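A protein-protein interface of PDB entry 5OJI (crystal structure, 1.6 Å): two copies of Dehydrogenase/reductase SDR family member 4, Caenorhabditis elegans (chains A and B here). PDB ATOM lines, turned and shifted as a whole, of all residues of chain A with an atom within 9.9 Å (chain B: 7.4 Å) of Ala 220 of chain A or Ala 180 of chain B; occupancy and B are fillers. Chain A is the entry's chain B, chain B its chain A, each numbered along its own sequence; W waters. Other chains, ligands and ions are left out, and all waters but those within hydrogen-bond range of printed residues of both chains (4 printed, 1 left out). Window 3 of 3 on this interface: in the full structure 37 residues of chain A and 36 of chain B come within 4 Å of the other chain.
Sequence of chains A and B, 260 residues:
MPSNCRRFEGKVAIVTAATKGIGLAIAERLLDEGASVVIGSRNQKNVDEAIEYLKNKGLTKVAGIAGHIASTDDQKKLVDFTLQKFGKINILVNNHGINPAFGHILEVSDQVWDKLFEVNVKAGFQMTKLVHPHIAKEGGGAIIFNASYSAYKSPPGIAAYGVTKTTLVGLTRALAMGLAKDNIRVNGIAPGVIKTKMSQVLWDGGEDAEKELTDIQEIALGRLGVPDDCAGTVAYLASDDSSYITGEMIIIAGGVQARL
Water W4 lies within hydrogen-bond range of the side-chain amide oxygen of Asn 183 of chain B (2.8 Å) and the guanidinium group of Arg 223 of chain A (3.0 Å). Water W2 lies within hydrogen-bond range of the backbone carbonyl oxygen of Val 256 of chain A (2.9 Å), the backbone NH of Gly 255 of chain A (3.3 Å) and the backbone carbonyl oxygen of Thr 246 of chain B (3.4 Å). Water W1 lies within hydrogen-bond range of OH of Tyr 244 of chain B (2.9 Å) and O of Ala 253 of chain A (3.0 Å). Water W3 lies within hydrogen-bond range of O of Ala 180 of chain B and O of Leu 221 of chain A.
The side-chain sulfur of Met 177 of chain B sits at hydrogen-bond distance from the side-chain amide nitrogen of Gln 257 of chain A (3.6 Å). The backbone carbonyl oxygen of Arg 223 of chain A sits at hydrogen-bond distance from the side-chain hydroxyl of Tyr 244 of chain B (2.7 Å). O of Gly 255 of chain A lies close to SD of Met 177 of chain B, 3.5 Å away. N of Gly 254 of chain A lies within hydrogen-bond range of O of Tyr 244 of chain B.
The backbone carbonyl oxygen (O) of Gly 254 of chain A sits at hydrogen-bond distance from the backbone NH (N) of Ala 220 of chain A, at 3.1 Å. N of Val 186 of chain B sits at hydrogen-bond distance from OG1 of Thr 246 of chain B. The backbone NH (N) of Leu 221 of chain A lies within hydrogen-bond range of the backbone carbonyl oxygen (O) of Gly 254 of chain A (3.0 Å). The backbone carbonyl oxygen of Thr 214 of chain A lies within hydrogen-bond range of the backbone NH of Ile 219 of chain A (2.8 Å).
Of the printed residues of chain B, Ala 220 of chain A touches Met 177 and Ala 180. Ala 180 of chain B touches one residue of chain A. Of the printed residues of chain B, Leu 224 of chain A touches Tyr 244 (3.4 Å). Of the printed residues of chain A, Met 177 of chain B touches Ala 220, Gly 255 and Gln 257. Leu 179 of chain B touches none of the printed residues of chain A. The nearest printed residue of chain B that does not touch Ile 219 of chain A is Ala 180 of chain B (6.3 Å).
Ile 219 of chain A touches Tyr 244 of chain B. Met 177 of chain B touches Ala 220 of chain A. Ala 180 of chain B touches Ala 220 of chain A. Thr 246 of chain B touches Leu 221 of chain A. Leu 224 of chain A touches Tyr 244 of chain B (C to OH, 3.4 Å). Ala 253 of chain A touches Tyr 244 of chain B (C to CE2, 3.5 Å). CG2 of Thr 246 of chain B touches O of Gly 254 of chain A (3.98 Å). CG2 of Thr 246 of chain B touches CA of Gly 255 of chain A (3.5 Å).
Among the printed residues, 12 pairs touch across the chains. Among the printed residues, no Asp or Glu carboxylate lies within 4 Å of a Lys or Arg side-chain nitrogen of the other chain.
No position is printed for both chains.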
ATOM      1  N   LYS A 211      21.277 -27.038  14.282  1.00  0.00           N
ATOM      2  CA  LYS A 211      22.014 -25.787  14.443  1.00  0.00           C
ATOM      3  C   LYS A 211      23.471 -26.054  14.803  1.00  0.00           C
ATOM      4  O   LYS A 211      24.378 -25.366  14.314  1.00  0.00           O
ATOM      5  CB  LYS A 211      21.335 -24.937  15.517  1.00  0.00           C
ATOM      6  CG  LYS A 211      21.564 -23.441  15.409  1.00  0.00           C
ATOM      7  CD  LYS A 211      20.431 -22.698  16.107  1.00  0.00           C
ATOM      8  CE  LYS A 211      20.614 -21.190  16.069  1.00  0.00           C
ATOM      9  NZ  LYS A 211      20.646 -20.655  14.679  1.00  0.00           N
ATOM     10  N   LEU A 213      25.087 -28.831  13.934  1.00  0.00           N
ATOM     11  CA  LEU A 213      25.707 -29.400  12.742  1.00  0.00           C
ATOM     12  C   LEU A 213      26.068 -28.312  11.735  1.00  0.00           C
ATOM     13  O   LEU A 213      27.114 -28.395  11.078  1.00  0.00           O
ATOM     14  CB  LEU A 213      24.783 -30.442  12.107  1.00  0.00           C
ATOM     15  CG  LEU A 213      25.384 -31.186  10.909  1.00  0.00           C
ATOM     16  CD1 LEU A 213      26.568 -32.044  11.337  1.00  0.00           C
ATOM     17  CD2 LEU A 213      24.341 -32.035  10.194  1.00  0.00           C
ATOM     18  N   THR A 214      25.225 -27.277  11.604  1.00  0.00           N
ATOM     19  CA  THR A 214      25.523 -26.210  10.649  1.00  0.00           C
ATOM     20  C   THR A 214      26.804 -25.477  11.012  1.00  0.00           C
ATOM     21  O   THR A 214      27.514 -24.994  10.124  1.00  0.00           O
ATOM     22  CB  THR A 214      24.369 -25.202  10.562  1.00  0.00           C
ATOM     23  OG1 THR A 214      24.204 -24.533  11.818  1.00  0.00           O
ATOM     24  CG2 THR A 214      23.067 -25.889  10.158  1.00  0.00           C
ATOM     25  N   ASP A 215      27.111 -25.372  12.306  1.00  0.00           N
ATOM     26  CA  ASP A 215      28.345 -24.716  12.723  1.00  0.00           C
ATOM     27  C   ASP A 215      29.550 -25.634  12.536  1.00  0.00           C
ATOM     28  O   ASP A 215      30.608 -25.182  12.085  1.00  0.00           O
ATOM     29  CB  ASP A 215      28.227 -24.253  14.178  1.00  0.00           C
ATOM     30  CG  ASP A 215      26.998 -23.381  14.418  1.00  0.00           C
ATOM     31  OD1 ASP A 215      26.558 -22.690  13.471  1.00  0.00           O
ATOM     32  OD2 ASP A 215      26.469 -23.392  15.549  1.00  0.00           O
ATOM     33  N   ILE A 216      29.406 -26.926  12.857  1.00  0.00           N
ATOM     34  CA  ILE A 216      30.482 -27.884  12.598  1.00  0.00           C
ATOM     35  C   ILE A 216      30.781 -27.946  11.107  1.00  0.00           C
ATOM     36  O   ILE A 216      31.939 -27.866  10.681  1.00  0.00           O
ATOM     37  CB  ILE A 216      30.118 -29.282  13.142  1.00  0.00           C
ATOM     38  CG1 ILE A 216      29.689 -29.233  14.614  1.00  0.00           C
ATOM     39  CG2 ILE A 216      31.295 -30.245  12.967  1.00  0.00           C
ATOM     40  CD1 ILE A 216      30.539 -28.349  15.502  1.00  0.00           C
ATOM     41  N   GLN A 217      29.738 -28.126  10.295  1.00  0.00           N
ATOM     42  CA  GLN A 217      29.878 -28.163   8.846  1.00  0.00           C
ATOM     43  C   GLN A 217      30.298 -26.822   8.258  1.00  0.00           C
ATOM     44  O   GLN A 217      30.639 -26.768   7.071  1.00  0.00           O
ATOM     45  CB  GLN A 217      28.556 -28.603   8.218  1.00  0.00           C
ATOM     46  CG  GLN A 217      28.186 -30.035   8.512  1.00  0.00           C
ATOM     47  CD  GLN A 217      29.030 -31.014   7.731  1.00  0.00           C
ATOM     48  OE1 GLN A 217      29.435 -30.739   6.597  1.00  0.00           O
ATOM     49  NE2 GLN A 217      29.307 -32.164   8.332  1.00  0.00           N
ATOM     50  N   GLU A 218      30.263 -25.748   9.046  1.00  0.00           N
ATOM     51  CA  GLU A 218      30.605 -24.409   8.571  1.00  0.00           C
ATOM     52  C   GLU A 218      29.709 -23.993   7.406  1.00  0.00           C
ATOM     53  O   GLU A 218      30.185 -23.606   6.339  1.00  0.00           O
ATOM     54  CB  GLU A 218      32.080 -24.331   8.170  1.00  0.00           C
ATOM     55  CG  GLU A 218      33.052 -24.586   9.306  1.00  0.00           C
ATOM     56  CD  GLU A 218      34.495 -24.439   8.863  1.00  0.00           C
ATOM     57  OE1 GLU A 218      35.020 -23.303   8.912  1.00  0.00           O
ATOM     58  OE2 GLU A 218      35.092 -25.458   8.449  1.00  0.00           O
ATOM     59  N   ILE A 219      28.397 -24.065   7.618  1.00  0.00           N
ATOM     60  CA  ILE A 219      27.427 -23.697   6.591  1.00  0.00           C
ATOM     61  C   ILE A 219      27.083 -22.226   6.778  1.00  0.00           C
ATOM     62  O   ILE A 219      26.384 -21.859   7.726  1.00  0.00           O
ATOM     63  CB  ILE A 219      26.167 -24.571   6.654  1.00  0.00           C
ATOM     64  CG1 ILE A 219      26.540 -26.057   6.586  1.00  0.00           C
ATOM     65  CG2 ILE A 219      25.232 -24.178   5.526  1.00  0.00           C
ATOM     66  CD1 ILE A 219      25.368 -26.999   6.747  1.00  0.00           C
ATOM     67  N   ALA A 220      27.534 -21.391   5.841  1.00  0.00           N
ATOM     68  CA  ALA A 220      27.403 -19.947   5.994  1.00  0.00           C
ATOM     69  C   ALA A 220      25.955 -19.536   6.210  1.00  0.00           C
ATOM     70  O   ALA A 220      25.674 -18.681   7.052  1.00  0.00           O
ATOM     71  CB  ALA A 220      27.996 -19.234   4.775  1.00  0.00           C
ATOM     72  N   LEU A 221      25.022 -20.126   5.461  1.00  0.00           N
ATOM     73  CA  LEU A 221      23.622 -19.725   5.532  1.00  0.00           C
ATOM     74  C   LEU A 221      22.915 -20.254   6.778  1.00  0.00           C
ATOM     75  O   LEU A 221      21.757 -19.896   7.010  1.00  0.00           O
ATOM     76  CB  LEU A 221      22.872 -20.176   4.273  1.00  0.00           C
ATOM     77  CG  LEU A 221      23.326 -19.508   2.962  1.00  0.00           C
ATOM     78  CD1 LEU A 221      22.513 -20.023   1.793  1.00  0.00           C
ATOM     79  CD2 LEU A 221      23.229 -17.983   3.030  1.00  0.00           C
ATOM     80  N   GLY A 222      23.577 -21.079   7.582  1.00  0.00           N
ATOM     81  CA  GLY A 222      23.084 -21.369   8.916  1.00  0.00           C
ATOM     82  C   GLY A 222      21.913 -22.318   8.987  1.00  0.00           C
ATOM     83  O   GLY A 222      21.169 -22.296   9.970  1.00  0.00           O
ATOM     84  N   ARG A 223      21.717 -23.156   7.976  1.00  0.00           N
ATOM     85  CA  ARG A 223      20.652 -24.143   8.023  1.00  0.00           C
ATOM     86  C   ARG A 223      21.053 -25.319   7.152  1.00  0.00           C
ATOM     87  O   ARG A 223      21.937 -25.211   6.297  1.00  0.00           O
ATOM     88  CB  ARG A 223      19.316 -23.567   7.545  1.00  0.00           C
ATOM     89  CG  ARG A 223      19.318 -23.199   6.080  1.00  0.00           C
ATOM     90  CD  ARG A 223      17.965 -22.708   5.622  1.00  0.00           C
ATOM     91  NE  ARG A 223      17.957 -22.443   4.187  1.00  0.00           N
ATOM     92  CZ  ARG A 223      18.436 -21.342   3.615  1.00  0.00           C
ATOM     93  NH1 ARG A 223      18.978 -20.371   4.345  1.00  0.00           N
ATOM     94  NH2 ARG A 223      18.371 -21.213   2.296  1.00  0.00           N
ATOM     95  N   LEU A 224      20.394 -26.448   7.383  1.00  0.00           N
ATOM     96  CA  LEU A 224      20.596 -27.599   6.527  1.00  0.00           C
ATOM     97  C   LEU A 224      19.744 -27.455   5.280  1.00  0.00           C
ATOM     98  O   LEU A 224      18.774 -26.694   5.242  1.00  0.00           O
ATOM     99  CB  LEU A 224      20.223 -28.895   7.242  1.00  0.00           C
ATOM    100  CG  LEU A 224      20.913 -29.117   8.578  1.00  0.00           C
ATOM    101  CD1 LEU A 224      20.364 -30.379   9.213  1.00  0.00           C
ATOM    102  CD2 LEU A 224      22.430 -29.190   8.402  1.00  0.00           C
ATOM    103  N   ALA A 253      25.313 -26.251  -0.985  1.00  0.00           N
ATOM    104  CA  ALA A 253      25.676 -26.620   0.375  1.00  0.00           C
ATOM    105  C   ALA A 253      25.596 -25.428   1.323  1.00  0.00           C
ATOM    106  O   ALA A 253      26.230 -25.453   2.372  1.00  0.00           O
ATOM    107  CB  ALA A 253      27.082 -27.234   0.400  1.00  0.00           C
ATOM    108  N   GLY A 254      24.835 -24.394   0.980  1.00  0.00           N
ATOM    109  CA  GLY A 254      24.657 -23.247   1.854  1.00  0.00           C
ATOM    110  C   GLY A 254      25.910 -22.461   2.161  1.00  0.00           C
ATOM    111  O   GLY A 254      25.968 -21.785   3.193  1.00  0.00           O
ATOM    112  N   GLY A 255      26.913 -22.520   1.293  1.00  0.00           N
ATOM    113  CA  GLY A 255      28.122 -21.748   1.469  1.00  0.00           C
ATOM    114  C   GLY A 255      29.279 -22.462   2.138  1.00  0.00           C
ATOM    115  O   GLY A 255      30.186 -21.786   2.632  1.00  0.00           O
ATOM    116  N   VAL A 256      29.274 -23.797   2.190  1.00  0.00           N
ATOM    117  CA  VAL A 256      30.462 -24.514   2.642  1.00  0.00           C
ATOM    118  C   VAL A 256      31.519 -24.445   1.550  1.00  0.00           C
ATOM    119  O   VAL A 256      31.220 -24.623   0.361  1.00  0.00           O
ATOM    120  CB  VAL A 256      30.143 -25.975   3.008  1.00  0.00           C
ATOM    121  CG1 VAL A 256      31.355 -26.613   3.664  1.00  0.00           C
ATOM    122  CG2 VAL A 256      28.973 -26.065   3.964  1.00  0.00           C
ATOM    123  N   GLN A 257      32.764 -24.212   1.951  1.00  0.00           N
ATOM    124  CA  GLN A 257      33.861 -23.936   1.030  1.00  0.00           C
ATOM    125  C   GLN A 257      34.712 -25.178   0.786  1.00  0.00           C
ATOM    126  O   GLN A 257      35.252 -25.755   1.737  1.00  0.00           O
ATOM    127  CB  GLN A 257      34.762 -22.841   1.594  1.00  0.00           C
ATOM    128  CG  GLN A 257      34.050 -21.554   1.971  1.00  0.00           C
ATOM    129  CD  GLN A 257      35.029 -20.444   2.290  1.00  0.00           C
ATOM    130  OE1 GLN A 257      35.737 -19.950   1.412  1.00  0.00           O
ATOM    131  NE2 GLN A 257      35.092 -20.064   3.556  1.00  0.00           N
ATOM    132  N   ALA B 174      34.413 -14.133  -0.395  1.00  0.00           N
ATOM    133  CA  ALA B 174      34.550 -13.387   0.852  1.00  0.00           C
ATOM    134  C   ALA B 174      33.243 -12.710   1.224  1.00  0.00           C
ATOM    135  O   ALA B 174      32.811 -12.767   2.383  1.00  0.00           O
ATOM    136  CB  ALA B 174      35.669 -12.349   0.727  1.00  0.00           C
ATOM    137  N   LEU B 175      32.602 -12.054   0.254  1.00  0.00           N
ATOM    138  CA  LEU B 175      31.335 -11.398   0.532  1.00  0.00           C
ATOM    139  C   LEU B 175      30.239 -12.414   0.816  1.00  0.00           C
ATOM    140  O   LEU B 175      29.357 -12.158   1.640  1.00  0.00           O
ATOM    141  CB  LEU B 175      30.944 -10.498  -0.637  1.00  0.00           C
ATOM    142  CG  LEU B 175      31.873  -9.296  -0.859  1.00  0.00           C
ATOM    143  CD1 LEU B 175      31.564  -8.585  -2.145  1.00  0.00           C
ATOM    144  CD2 LEU B 175      31.753  -8.345   0.308  1.00  0.00           C
ATOM    145  N   ALA B 176      30.256 -13.564   0.132  1.00  0.00           N
ATOM    146  CA  ALA B 176      29.296 -14.613   0.463  1.00  0.00           C
ATOM    147  C   ALA B 176      29.423 -15.006   1.926  1.00  0.00           C
ATOM    148  O   ALA B 176      28.421 -15.086   2.652  1.00  0.00           O
ATOM    149  CB  ALA B 176      29.500 -15.831  -0.435  1.00  0.00           C
ATOM    150  N   MET B 177      30.652 -15.247   2.385  1.00  0.00           N
ATOM    151  CA  MET B 177      30.838 -15.667   3.765  1.00  0.00           C
ATOM    152  C   MET B 177      30.422 -14.562   4.732  1.00  0.00           C
ATOM    153  O   MET B 177      29.822 -14.845   5.774  1.00  0.00           O
ATOM    154  CB  MET B 177      32.290 -16.079   4.008  1.00  0.00           C
ATOM    155  CG  MET B 177      32.784 -17.269   3.168  1.00  0.00           C
ATOM    156  SD  MET B 177      31.752 -18.756   3.274  1.00  0.00           S
ATOM    157  CE  MET B 177      30.659 -18.543   1.876  1.00  0.00           C
ATOM    158  N   GLY B 178      30.721 -13.299   4.401  1.00  0.00           N
ATOM    159  CA  GLY B 178      30.449 -12.196   5.313  1.00  0.00           C
ATOM    160  C   GLY B 178      29.026 -11.698   5.313  1.00  0.00           C
ATOM    161  O   GLY B 178      28.594 -11.103   6.306  1.00  0.00           O
ATOM    162  N   LEU B 179      28.292 -11.894   4.225  1.00  0.00           N
ATOM    163  CA  LEU B 179      26.935 -11.381   4.117  1.00  0.00           C
ATOM    164  C   LEU B 179      25.873 -12.453   4.338  1.00  0.00           C
ATOM    165  O   LEU B 179      24.679 -12.134   4.313  1.00  0.00           O
ATOM    166  CB  LEU B 179      26.743 -10.711   2.757  1.00  0.00           C
ATOM    167  CG  LEU B 179      27.280  -9.278   2.649  1.00  0.00           C
ATOM    168  CD1 LEU B 179      28.718  -9.136   3.120  1.00  0.00           C
ATOM    169  CD2 LEU B 179      27.145  -8.789   1.216  1.00  0.00           C
ATOM    170  N   ALA B 180      26.285 -13.700   4.595  1.00  0.00           N
ATOM    171  CA  ALA B 180      25.332 -14.766   4.896  1.00  0.00           C
ATOM    172  C   ALA B 180      24.465 -14.415   6.099  1.00  0.00           C
ATOM    173  O   ALA B 180      23.270 -14.740   6.135  1.00  0.00           O
ATOM    174  CB  ALA B 180      26.090 -16.066   5.147  1.00  0.00           C
ATOM    175  N   LYS B 181      25.050 -13.748   7.096  1.00  0.00           N
ATOM    176  CA  LYS B 181      24.303 -13.372   8.294  1.00  0.00           C
ATOM    177  C   LYS B 181      23.079 -12.528   7.964  1.00  0.00           C
ATOM    178  O   LYS B 181      22.116 -12.501   8.741  1.00  0.00           O
ATOM    179  CB  LYS B 181      25.210 -12.608   9.266  1.00  0.00           C
ATOM    180  CG  LYS B 181      25.697 -11.251   8.749  1.00  0.00           C
ATOM    181  CD  LYS B 181      26.501 -10.472   9.798  1.00  0.00           C
ATOM    182  CE  LYS B 181      27.138  -9.209   9.191  1.00  0.00           C
ATOM    183  NZ  LYS B 181      26.146  -8.287   8.546  1.00  0.00           N
ATOM    184  N   ASP B 182      23.106 -11.811   6.843  1.00  0.00           N
ATOM    185  CA  ASP B 182      21.992 -10.984   6.408  1.00  0.00           C
ATOM    186  C   ASP B 182      21.134 -11.675   5.358  1.00  0.00           C
ATOM    187  O   ASP B 182      20.283 -11.026   4.744  1.00  0.00           O
ATOM    188  CB  ASP B 182      22.509  -9.658   5.866  1.00  0.00           C
ATOM    189  CG  ASP B 182      23.300  -8.882   6.895  1.00  0.00           C
ATOM    190  OD1 ASP B 182      22.776  -8.670   8.000  1.00  0.00           O
ATOM    191  OD2 ASP B 182      24.452  -8.506   6.602  1.00  0.00           O
ATOM    192  N   ASN B 183      21.334 -12.973   5.152  1.00  0.00           N
ATOM    193  CA  ASN B 183      20.622 -13.725   4.129  1.00  0.00           C
ATOM    194  C   ASN B 183      20.837 -13.107   2.753  1.00  0.00           C
ATOM    195  O   ASN B 183      19.933 -13.090   1.914  1.00  0.00           O
ATOM    196  CB  ASN B 183      19.129 -13.819   4.451  1.00  0.00           C
ATOM    197  CG  ASN B 183      18.405 -14.802   3.557  1.00  0.00           C
ATOM    198  OD1 ASN B 183      18.958 -15.841   3.184  1.00  0.00           O
ATOM    199  ND2 ASN B 183      17.171 -14.472   3.188  1.00  0.00           N
ATOM    200  N   ILE B 184      22.042 -12.590   2.508  1.00  0.00           N
ATOM    201  CA  ILE B 184      22.420 -12.080   1.192  1.00  0.00           C
ATOM    202  C   ILE B 184      23.385 -13.077   0.571  1.00  0.00           C
ATOM    203  O   ILE B 184      24.493 -13.292   1.085  1.00  0.00           O
ATOM    204  CB  ILE B 184      23.044 -10.679   1.255  1.00  0.00           C
ATOM    205  CG1 ILE B 184      22.067  -9.694   1.911  1.00  0.00           C
ATOM    206  CG2 ILE B 184      23.419 -10.218  -0.157  1.00  0.00           C
ATOM    207  CD1 ILE B 184      22.658  -8.315   2.161  1.00  0.00           C
ATOM    208  N   ARG B 185      22.955 -13.684  -0.529  1.00  0.00           N
ATOM    209  CA  ARG B 185      23.725 -14.694  -1.240  1.00  0.00           C
ATOM    210  C   ARG B 185      24.548 -13.985  -2.303  1.00  0.00           C
ATOM    211  O   ARG B 185      24.026 -13.137  -3.025  1.00  0.00           O
ATOM    212  CB  ARG B 185      22.785 -15.746  -1.858  1.00  0.00           C
ATOM    213  CG  ARG B 185      21.989 -16.548  -0.815  1.00  0.00           C
ATOM    214  CD  ARG B 185      21.106 -17.647  -1.443  1.00  0.00           C
ATOM    215  NE  ARG B 185      20.119 -17.109  -2.370  1.00  0.00           N
ATOM    216  CZ  ARG B 185      20.266 -17.049  -3.687  1.00  0.00           C
ATOM    217  NH1 ARG B 185      21.370 -17.500  -4.267  1.00  0.00           N
ATOM    218  NH2 ARG B 185      19.310 -16.518  -4.436  1.00  0.00           N
ATOM    219  N   VAL B 186      25.836 -14.315  -2.373  1.00  0.00           N
ATOM    220  CA  VAL B 186      26.768 -13.703  -3.307  1.00  0.00           C
ATOM    221  C   VAL B 186      27.339 -14.814  -4.178  1.00  0.00           C
ATOM    222  O   VAL B 186      27.959 -15.754  -3.671  1.00  0.00           O
ATOM    223  CB  VAL B 186      27.892 -12.940  -2.577  1.00  0.00           C
ATOM    224  CG1 VAL B 186      28.736 -12.187  -3.569  1.00  0.00           C
ATOM    225  CG2 VAL B 186      27.318 -12.006  -1.509  1.00  0.00           C
ATOM    226  N   TYR B 244      19.888 -22.032  -1.572  1.00  0.00           N
ATOM    227  CA  TYR B 244      20.873 -22.680  -0.711  1.00  0.00           C
ATOM    228  C   TYR B 244      22.272 -22.616  -1.313  1.00  0.00           C
ATOM    229  O   TYR B 244      23.140 -23.422  -0.955  1.00  0.00           O
ATOM    230  CB  TYR B 244      20.459 -24.129  -0.428  1.00  0.00           C
ATOM    231  CG  TYR B 244      21.092 -24.761   0.783  1.00  0.00           C
ATOM    232  CD1 TYR B 244      21.002 -24.165   2.037  1.00  0.00           C
ATOM    233  CD2 TYR B 244      21.755 -25.975   0.685  1.00  0.00           C
ATOM    234  CE1 TYR B 244      21.561 -24.746   3.144  1.00  0.00           C
ATOM    235  CE2 TYR B 244      22.312 -26.573   1.796  1.00  0.00           C
ATOM    236  CZ  TYR B 244      22.219 -25.948   3.021  1.00  0.00           C
ATOM    237  OH  TYR B 244      22.786 -26.539   4.120  1.00  0.00           O
ATOM    238  N   THR B 246      25.574 -20.135  -2.181  1.00  0.00           N
ATOM    239  CA  THR B 246      26.274 -18.875  -2.008  1.00  0.00           C
ATOM    240  C   THR B 246      27.769 -19.148  -2.051  1.00  0.00           C
ATOM    241  O   THR B 246      28.235 -20.242  -1.702  1.00  0.00           O
ATOM    242  CB  THR B 246      25.845 -18.161  -0.711  1.00  0.00           C
ATOM    243  OG1 THR B 246      26.287 -16.796  -0.744  1.00  0.00           O
ATOM    244  CG2 THR B 246      26.394 -18.854   0.528  1.00  0.00           C
HETATM  245  O   HOH W   1      25.184 -28.007   3.435  1.00  0.00           O
HETATM  246  O   HOH W   2      28.997 -23.447  -1.049  1.00  0.00           O
HETATM  247  O   HOH W   3      21.765 -16.790   8.006  1.00  0.00           O
HETATM  248  O   HOH W   4      18.850 -18.286   1.856  1.00  0.00           O
